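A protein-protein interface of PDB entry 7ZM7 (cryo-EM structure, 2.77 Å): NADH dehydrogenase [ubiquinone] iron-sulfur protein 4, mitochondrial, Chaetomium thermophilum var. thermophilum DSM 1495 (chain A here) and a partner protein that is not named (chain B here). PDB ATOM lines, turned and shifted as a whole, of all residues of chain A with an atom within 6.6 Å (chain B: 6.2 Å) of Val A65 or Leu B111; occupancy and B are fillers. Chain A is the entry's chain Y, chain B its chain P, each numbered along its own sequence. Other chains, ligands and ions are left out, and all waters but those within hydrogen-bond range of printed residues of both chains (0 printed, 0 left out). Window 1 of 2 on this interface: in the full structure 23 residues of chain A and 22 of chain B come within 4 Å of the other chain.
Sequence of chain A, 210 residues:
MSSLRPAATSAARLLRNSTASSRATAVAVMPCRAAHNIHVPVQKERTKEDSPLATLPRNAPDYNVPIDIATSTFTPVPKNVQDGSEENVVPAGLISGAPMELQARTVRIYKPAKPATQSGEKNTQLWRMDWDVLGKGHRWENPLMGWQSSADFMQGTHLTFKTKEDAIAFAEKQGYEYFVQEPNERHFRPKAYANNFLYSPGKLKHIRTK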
ATOM      1  N   PRO A  61       7.681  19.115  20.522  1.00  0.00           N
ATOM      2  CA  PRO A  61       7.919  18.879  19.096  1.00  0.00           C
ATOM      3  C   PRO A  61       7.756  17.404  18.763  1.00  0.00           C
ATOM      4  O   PRO A  61       8.442  16.552  19.324  1.00  0.00           O
ATOM      5  CB  PRO A  61       9.364  19.348  18.901  1.00  0.00           C
ATOM      6  CG  PRO A  61       9.988  19.199  20.224  1.00  0.00           C
ATOM      7  CD  PRO A  61       8.916  19.485  21.230  1.00  0.00           C
ATOM      8  N   ASP A  62       6.848  17.102  17.844  1.00  0.00           N
ATOM      9  CA  ASP A  62       6.608  15.721  17.442  1.00  0.00           C
ATOM     10  C   ASP A  62       7.773  15.279  16.584  1.00  0.00           C
ATOM     11  O   ASP A  62       7.746  15.414  15.359  1.00  0.00           O
ATOM     12  CB  ASP A  62       5.290  15.583  16.695  1.00  0.00           C
ATOM     13  CG  ASP A  62       4.744  14.162  16.730  1.00  0.00           C
ATOM     14  OD1 ASP A  62       4.560  13.619  17.840  1.00  0.00           O
ATOM     15  OD2 ASP A  62       4.487  13.590  15.649  1.00  0.00           O
ATOM     16  N   TYR A  63       8.796  14.724  17.236  1.00  0.00           N
ATOM     17  CA  TYR A  63       9.995  14.263  16.553  1.00  0.00           C
ATOM     18  C   TYR A  63       9.726  13.076  15.653  1.00  0.00           C
ATOM     19  O   TYR A  63      10.608  12.702  14.875  1.00  0.00           O
ATOM     20  CB  TYR A  63      11.074  13.896  17.561  1.00  0.00           C
ATOM     21  CG  TYR A  63      11.800  15.063  18.166  1.00  0.00           C
ATOM     22  CD1 TYR A  63      12.600  15.879  17.399  1.00  0.00           C
ATOM     23  CD2 TYR A  63      11.716  15.322  19.521  1.00  0.00           C
ATOM     24  CE1 TYR A  63      13.270  16.938  17.954  1.00  0.00           C
ATOM     25  CE2 TYR A  63      12.387  16.369  20.084  1.00  0.00           C
ATOM     26  CZ  TYR A  63      13.162  17.179  19.297  1.00  0.00           C
ATOM     27  OH  TYR A  63      13.821  18.236  19.864  1.00  0.00           O
ATOM     28  N   ASN A  64       8.543  12.472  15.736  1.00  0.00           N
ATOM     29  CA  ASN A  64       8.211  11.305  14.937  1.00  0.00           C
ATOM     30  C   ASN A  64       7.207  11.607  13.837  1.00  0.00           C
ATOM     31  O   ASN A  64       6.532  10.691  13.363  1.00  0.00           O
ATOM     32  CB  ASN A  64       7.674  10.181  15.824  1.00  0.00           C
ATOM     33  CG  ASN A  64       8.733   9.595  16.723  1.00  0.00           C
ATOM     34  OD1 ASN A  64       8.527   9.442  17.924  1.00  0.00           O
ATOM     35  ND2 ASN A  64       9.881   9.269  16.147  1.00  0.00           N
ATOM     36  N   VAL A  65       7.084  12.859  13.420  1.00  0.00           N
ATOM     37  CA  VAL A  65       6.231  13.170  12.280  1.00  0.00           C
ATOM     38  C   VAL A  65       6.777  12.431  11.068  1.00  0.00           C
ATOM     39  O   VAL A  65       8.002  12.326  10.904  1.00  0.00           O
ATOM     40  CB  VAL A  65       6.175  14.675  12.001  1.00  0.00           C
ATOM     41  CG1 VAL A  65       5.334  15.379  13.028  1.00  0.00           C
ATOM     42  CG2 VAL A  65       7.570  15.235  11.980  1.00  0.00           C
ATOM     43  N   PRO A  66       5.926  11.906  10.206  1.00  0.00           N
ATOM     44  CA  PRO A  66       6.420  11.305   8.964  1.00  0.00           C
ATOM     45  C   PRO A  66       6.818  12.369   7.958  1.00  0.00           C
ATOM     46  O   PRO A  66       5.980  13.166   7.531  1.00  0.00           O
ATOM     47  CB  PRO A  66       5.230  10.475   8.474  1.00  0.00           C
ATOM     48  CG  PRO A  66       4.036  11.088   9.109  1.00  0.00           C
ATOM     49  CD  PRO A  66       4.463  11.829  10.336  1.00  0.00           C
ATOM     50  N   ILE A  67       8.096  12.391   7.579  1.00  0.00           N
ATOM     51  CA  ILE A  67       8.601  13.387   6.642  1.00  0.00           C
ATOM     52  C   ILE A  67       8.038  13.126   5.253  1.00  0.00           C
ATOM     53  O   ILE A  67       7.410  12.091   5.002  1.00  0.00           O
ATOM     54  CB  ILE A  67      10.136  13.357   6.609  1.00  0.00           C
ATOM     55  CG1 ILE A  67      10.611  11.997   6.115  1.00  0.00           C
ATOM     56  CG2 ILE A  67      10.706  13.634   7.987  1.00  0.00           C
ATOM     57  CD1 ILE A  67      12.066  11.937   5.828  1.00  0.00           C
ATOM     58  N   THR A  71      11.142  17.366   2.697  1.00  0.00           N
ATOM     59  CA  THR A  71      11.795  17.551   3.986  1.00  0.00           C
ATOM     60  C   THR A  71      13.307  17.471   3.833  1.00  0.00           C
ATOM     61  O   THR A  71      13.828  16.626   3.106  1.00  0.00           O
ATOM     62  CB  THR A  71      11.298  16.517   4.992  1.00  0.00           C
ATOM     63  OG1 THR A  71       9.905  16.722   5.224  1.00  0.00           O
ATOM     64  CG2 THR A  71      12.022  16.652   6.309  1.00  0.00           C
ATOM     65  N   SER A  72      14.005  18.364   4.521  1.00  0.00           N
ATOM     66  CA  SER A  72      15.431  18.565   4.320  1.00  0.00           C
ATOM     67  C   SER A  72      16.136  18.593   5.671  1.00  0.00           C
ATOM     68  O   SER A  72      15.544  18.344   6.724  1.00  0.00           O
ATOM     69  CB  SER A  72      15.658  19.857   3.534  1.00  0.00           C
ATOM     70  OG  SER A  72      14.810  20.880   4.009  1.00  0.00           O
ATOM     71  N   PHE A  74      17.198  21.305   6.810  1.00  0.00           N
ATOM     72  CA  PHE A  74      16.859  22.619   7.317  1.00  0.00           C
ATOM     73  C   PHE A  74      15.441  22.681   7.840  1.00  0.00           C
ATOM     74  O   PHE A  74      15.086  23.657   8.500  1.00  0.00           O
ATOM     75  CB  PHE A  74      17.049  23.669   6.223  1.00  0.00           C
ATOM     76  CG  PHE A  74      18.355  23.570   5.520  1.00  0.00           C
ATOM     77  CD1 PHE A  74      19.475  24.151   6.047  1.00  0.00           C
ATOM     78  CD2 PHE A  74      18.463  22.883   4.335  1.00  0.00           C
ATOM     79  CE1 PHE A  74      20.668  24.054   5.399  1.00  0.00           C
ATOM     80  CE2 PHE A  74      19.656  22.785   3.691  1.00  0.00           C
ATOM     81  CZ  PHE A  74      20.761  23.367   4.217  1.00  0.00           C
ATOM     82  N   THR A  75      14.634  21.671   7.569  1.00  0.00           N
ATOM     83  CA  THR A  75      13.264  21.620   8.041  1.00  0.00           C
ATOM     84  C   THR A  75      13.251  21.541   9.561  1.00  0.00           C
ATOM     85  O   THR A  75      13.908  20.668  10.127  1.00  0.00           O
ATOM     86  CB  THR A  75      12.559  20.417   7.446  1.00  0.00           C
ATOM     87  OG1 THR A  75      12.590  20.513   6.026  1.00  0.00           O
ATOM     88  CG2 THR A  75      11.130  20.361   7.891  1.00  0.00           C
ATOM     89  N   PRO A  76      12.552  22.425  10.252  1.00  0.00           N
ATOM     90  CA  PRO A  76      12.437  22.282  11.701  1.00  0.00           C
ATOM     91  C   PRO A  76      11.472  21.167  12.065  1.00  0.00           C
ATOM     92  O   PRO A  76      10.712  20.661  11.238  1.00  0.00           O
ATOM     93  CB  PRO A  76      11.914  23.644  12.145  1.00  0.00           C
ATOM     94  CG  PRO A  76      12.157  24.541  10.978  1.00  0.00           C
ATOM     95  CD  PRO A  76      11.993  23.701   9.794  1.00  0.00           C
ATOM     96  N   VAL A  77      11.535  20.757  13.326  1.00  0.00           N
ATOM     97  CA  VAL A  77      10.635  19.723  13.820  1.00  0.00           C
ATOM     98  C   VAL A  77       9.313  20.383  14.194  1.00  0.00           C
ATOM     99  O   VAL A  77       9.294  21.322  15.001  1.00  0.00           O
ATOM    100  CB  VAL A  77      11.248  18.955  15.003  1.00  0.00           C
ATOM    101  CG1 VAL A  77      10.222  18.025  15.622  1.00  0.00           C
ATOM    102  CG2 VAL A  77      12.456  18.160  14.550  1.00  0.00           C
ATOM    103  N   PRO A  78       8.199  19.949  13.624  1.00  0.00           N
ATOM    104  CA  PRO A  78       6.909  20.554  13.958  1.00  0.00           C
ATOM    105  C   PRO A  78       6.382  20.083  15.303  1.00  0.00           C
ATOM    106  O   PRO A  78       6.753  19.032  15.819  1.00  0.00           O
ATOM    107  CB  PRO A  78       6.003  20.086  12.822  1.00  0.00           C
ATOM    108  CG  PRO A  78       6.591  18.801  12.409  1.00  0.00           C
ATOM    109  CD  PRO A  78       8.062  18.884  12.623  1.00  0.00           C
ATOM    110  N   LYS A  79       5.502  20.900  15.873  1.00  0.00           N
ATOM    111  CA  LYS A  79       4.747  20.482  17.044  1.00  0.00           C
ATOM    112  C   LYS A  79       3.388  19.902  16.685  1.00  0.00           C
ATOM    113  O   LYS A  79       2.995  18.873  17.236  1.00  0.00           O
ATOM    114  CB  LYS A  79       4.557  21.647  18.005  1.00  0.00           C
ATOM    115  CG  LYS A  79       5.783  22.474  18.224  1.00  0.00           C
ATOM    116  CD  LYS A  79       5.543  23.516  19.280  1.00  0.00           C
ATOM    117  CE  LYS A  79       4.221  24.210  19.083  1.00  0.00           C
ATOM    118  NZ  LYS A  79       4.229  25.079  17.876  1.00  0.00           N
ATOM    119  N   ASN A  80       2.660  20.524  15.768  1.00  0.00           N
ATOM    120  CA  ASN A  80       1.309  20.100  15.434  1.00  0.00           C
ATOM    121  C   ASN A  80       1.151  20.049  13.926  1.00  0.00           C
ATOM    122  O   ASN A  80       1.513  20.996  13.228  1.00  0.00           O
ATOM    123  CB  ASN A  80       0.276  21.053  16.023  1.00  0.00           C
ATOM    124  CG  ASN A  80       0.429  21.217  17.495  1.00  0.00           C
ATOM    125  OD1 ASN A  80       0.765  22.292  17.979  1.00  0.00           O
ATOM    126  ND2 ASN A  80       0.189  20.147  18.230  1.00  0.00           N
ATOM    127  N   VAL A  81       0.616  18.949  13.430  1.00  0.00           N
ATOM    128  CA  VAL A  81       0.330  18.791  12.015  1.00  0.00           C
ATOM    129  C   VAL A  81      -1.166  18.592  11.879  1.00  0.00           C
ATOM    130  O   VAL A  81      -1.759  17.801  12.619  1.00  0.00           O
ATOM    131  CB  VAL A  81       1.116  17.617  11.409  1.00  0.00           C
ATOM    132  CG1 VAL A  81       0.610  17.302  10.032  1.00  0.00           C
ATOM    133  CG2 VAL A  81       2.584  17.952  11.369  1.00  0.00           C
ATOM    134  N   MET A 100       5.319  19.390   4.920  1.00  0.00           N
ATOM    135  CA  MET A 100       5.074  19.508   6.350  1.00  0.00           C
ATOM    136  C   MET A 100       5.763  20.718   6.962  1.00  0.00           C
ATOM    137  O   MET A 100       5.294  21.233   7.980  1.00  0.00           O
ATOM    138  CB  MET A 100       5.524  18.208   7.024  1.00  0.00           C
ATOM    139  CG  MET A 100       5.755  18.259   8.520  1.00  0.00           C
ATOM    140  SD  MET A 100       7.495  18.561   8.884  1.00  0.00           S
ATOM    141  CE  MET A 100       8.188  16.943   8.585  1.00  0.00           C
ATOM    142  N   GLU B 108      15.572   7.835   5.414  1.00  0.00           N
ATOM    143  CA  GLU B 108      14.395   8.109   6.222  1.00  0.00           C
ATOM    144  C   GLU B 108      14.719   9.038   7.381  1.00  0.00           C
ATOM    145  O   GLU B 108      13.951   9.963   7.658  1.00  0.00           O
ATOM    146  CB  GLU B 108      13.821   6.793   6.748  1.00  0.00           C
ATOM    147  CG  GLU B 108      12.527   6.919   7.522  1.00  0.00           C
ATOM    148  CD  GLU B 108      11.359   7.292   6.637  1.00  0.00           C
ATOM    149  OE1 GLU B 108      11.417   6.998   5.425  1.00  0.00           O
ATOM    150  OE2 GLU B 108      10.379   7.867   7.154  1.00  0.00           O
ATOM    151  N   LYS B 109      15.850   8.825   8.042  1.00  0.00           N
ATOM    152  CA  LYS B 109      16.289   9.674   9.144  1.00  0.00           C
ATOM    153  C   LYS B 109      16.706  11.014   8.557  1.00  0.00           C
ATOM    154  O   LYS B 109      17.850  11.194   8.134  1.00  0.00           O
ATOM    155  CB  LYS B 109      17.427   9.002   9.905  1.00  0.00           C
ATOM    156  CG  LYS B 109      17.991   9.803  11.064  1.00  0.00           C
ATOM    157  CD  LYS B 109      19.357  10.376  10.720  1.00  0.00           C
ATOM    158  CE  LYS B 109      20.344   9.268  10.393  1.00  0.00           C
ATOM    159  NZ  LYS B 109      21.678   9.800  10.008  1.00  0.00           N
ATOM    160  N   ARG B 110      15.766  11.958   8.511  1.00  0.00           N
ATOM    161  CA  ARG B 110      16.053  13.281   7.984  1.00  0.00           C
ATOM    162  C   ARG B 110      15.658  14.421   8.902  1.00  0.00           C
ATOM    163  O   ARG B 110      16.167  15.534   8.719  1.00  0.00           O
ATOM    164  CB  ARG B 110      15.382  13.482   6.622  1.00  0.00           C
ATOM    165  CG  ARG B 110      16.317  13.163   5.486  1.00  0.00           C
ATOM    166  CD  ARG B 110      15.704  13.519   4.184  1.00  0.00           C
ATOM    167  NE  ARG B 110      14.783  12.495   3.729  1.00  0.00           N
ATOM    168  CZ  ARG B 110      13.763  12.732   2.926  1.00  0.00           C
ATOM    169  NH1 ARG B 110      13.533  13.960   2.495  1.00  0.00           N
ATOM    170  NH2 ARG B 110      12.983  11.739   2.550  1.00  0.00           N
ATOM    171  N   LEU B 111      14.787  14.203   9.834  1.00  0.00           N
ATOM    172  CA  LEU B 111      14.679  15.120  10.943  1.00  0.00           C
ATOM    173  C   LEU B 111      15.600  14.666  12.061  1.00  0.00           C
ATOM    174  O   LEU B 111      15.927  13.484  12.156  1.00  0.00           O
ATOM    175  CB  LEU B 111      13.245  15.180  11.468  1.00  0.00           C
ATOM    176  CG  LEU B 111      12.200  15.973  10.684  1.00  0.00           C
ATOM    177  CD1 LEU B 111      10.958  16.152  11.512  1.00  0.00           C
ATOM    178  CD2 LEU B 111      12.740  17.310  10.258  1.00  0.00           C
ATOM    179  N   PRO B 112      16.060  15.571  12.913  1.00  0.00           N
ATOM    180  CA  PRO B 112      16.827  15.144  14.084  1.00  0.00           C
ATOM    181  C   PRO B 112      15.961  14.340  15.045  1.00  0.00           C
ATOM    182  O   PRO B 112      14.761  14.580  15.180  1.00  0.00           O
ATOM    183  CB  PRO B 112      17.285  16.466  14.698  1.00  0.00           C
ATOM    184  CG  PRO B 112      16.353  17.448  14.198  1.00  0.00           C
ATOM    185  CD  PRO B 112      15.941  17.030  12.846  1.00  0.00           C
ATOM    186  N   SER B 113      16.589  13.377  15.719  1.00  0.00           N
ATOM    187  CA  SER B 113      15.842  12.437  16.547  1.00  0.00           C
ATOM    188  C   SER B 113      15.301  13.097  17.804  1.00  0.00           C
ATOM    189  O   SER B 113      14.161  12.845  18.209  1.00  0.00           O
ATOM    190  CB  SER B 113      16.727  11.254  16.921  1.00  0.00           C
ATOM    191  OG  SER B 113      16.240  10.613  18.086  1.00  0.00           O
ATOM    192  N   ASN B 124      20.029  19.328  12.156  1.00  0.00           N
ATOM    193  CA  ASN B 124      20.077  18.211  11.157  1.00  0.00           C
ATOM    194  C   ASN B 124      21.075  18.495  10.024  1.00  0.00           C
ATOM    195  O   ASN B 124      21.609  17.543   9.465  1.00  0.00           O
ATOM    196  CB  ASN B 124      18.727  17.686  10.650  1.00  0.00           C
ATOM    197  CG  ASN B 124      18.829  16.242  10.211  1.00  0.00           C
ATOM    198  OD1 ASN B 124      18.921  15.953   9.022  1.00  0.00           O
ATOM    199  ND2 ASN B 124      18.856  15.330  11.168  1.00  0.00           N
ATOM    200  OXT ASN B 124      21.305  19.671   9.734  1.00  0.00           O
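The backbone carbonyl oxygen (O) of Thr A71 lies within hydrogen-bond range of the guanidinium group (NH1) of Arg B110 (2.8 Å).
The side-chain amide oxygen of Asn B124 sits close to the backbone carbonyl oxygen of Arg B110. The side-chain carboxylate (OD2) of Asp A62 sits close to the backbone NH (N) of Val A65 (3.5 Å). The backbone NH (N) of Ser A72 sits at hydrogen-bond distance from the side-chain hydroxyl (OG1) of Thr A75.
CD1 of Tyr A63 touches O of Pro B112, at 3.4 Å. Tyr A63 touches Ser B113 (CG to O, 3.2 Å). CD1 of Leu B111 touches CG2 of Val A65 (3.5 Å). Ile A67 touches Glu B108 (CD1 to O, 3.3 Å). Arg B110 touches Ile A67 (NH2 to CD1, 3.4 Å). CG2 of Ile A67 touches CG of Leu B111, at 3.9 Å. Arg B110 touches Ser A72 (O to O, 3.5 Å). CD2 of Leu B111 touches O of Thr A75, 3.6 Å away. CG2 of Val A77 touches CD1 of Leu B111, at 3.9 Å. Pro B112 touches Val A77.
Pro A61 touches none of the printed residues of chain B. Of chain B, only Leu B111 comes within 4 Å of Val A65. Printed residues of chain B within 4 Å of Ile A67: Glu B108 (3.3 Å), Arg B110 (3.4 Å) and Leu B111 (3.9 Å). Pro A78 touches none of the printed residues of chain B. Printed residues of chain A within 4 Å of Glu B108: Ile A67 (3.3 Å). Of chain A, only Val A65 (3.5 Å), Ile A67 (3.9 Å), Thr A75 (3.6 Å) and Val A77 (3.9 Å) come within 4 Å of Leu B111. Of the printed residues of chain A, Pro B112 touches Tyr A63 (3.4 Å) and Val A77 (3.98 Å). Of the printed residues of chain A, Ser B113 touches Tyr A63. The nearest printed residue of chain B that does not touch Thr A71 is Leu B111 (4.1 Å).
Of the 18 printed residues of chain A, 7 touch a printed residue of chain B. Printed residues of chain B that touch a printed residue of chain A: Glu B108, Arg B110, Leu B111, Pro B112 and Ser B113. Hydrophobic or aromatic side chains of chain B that line the printed part of chain A: Leu B111 and Pro B112.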
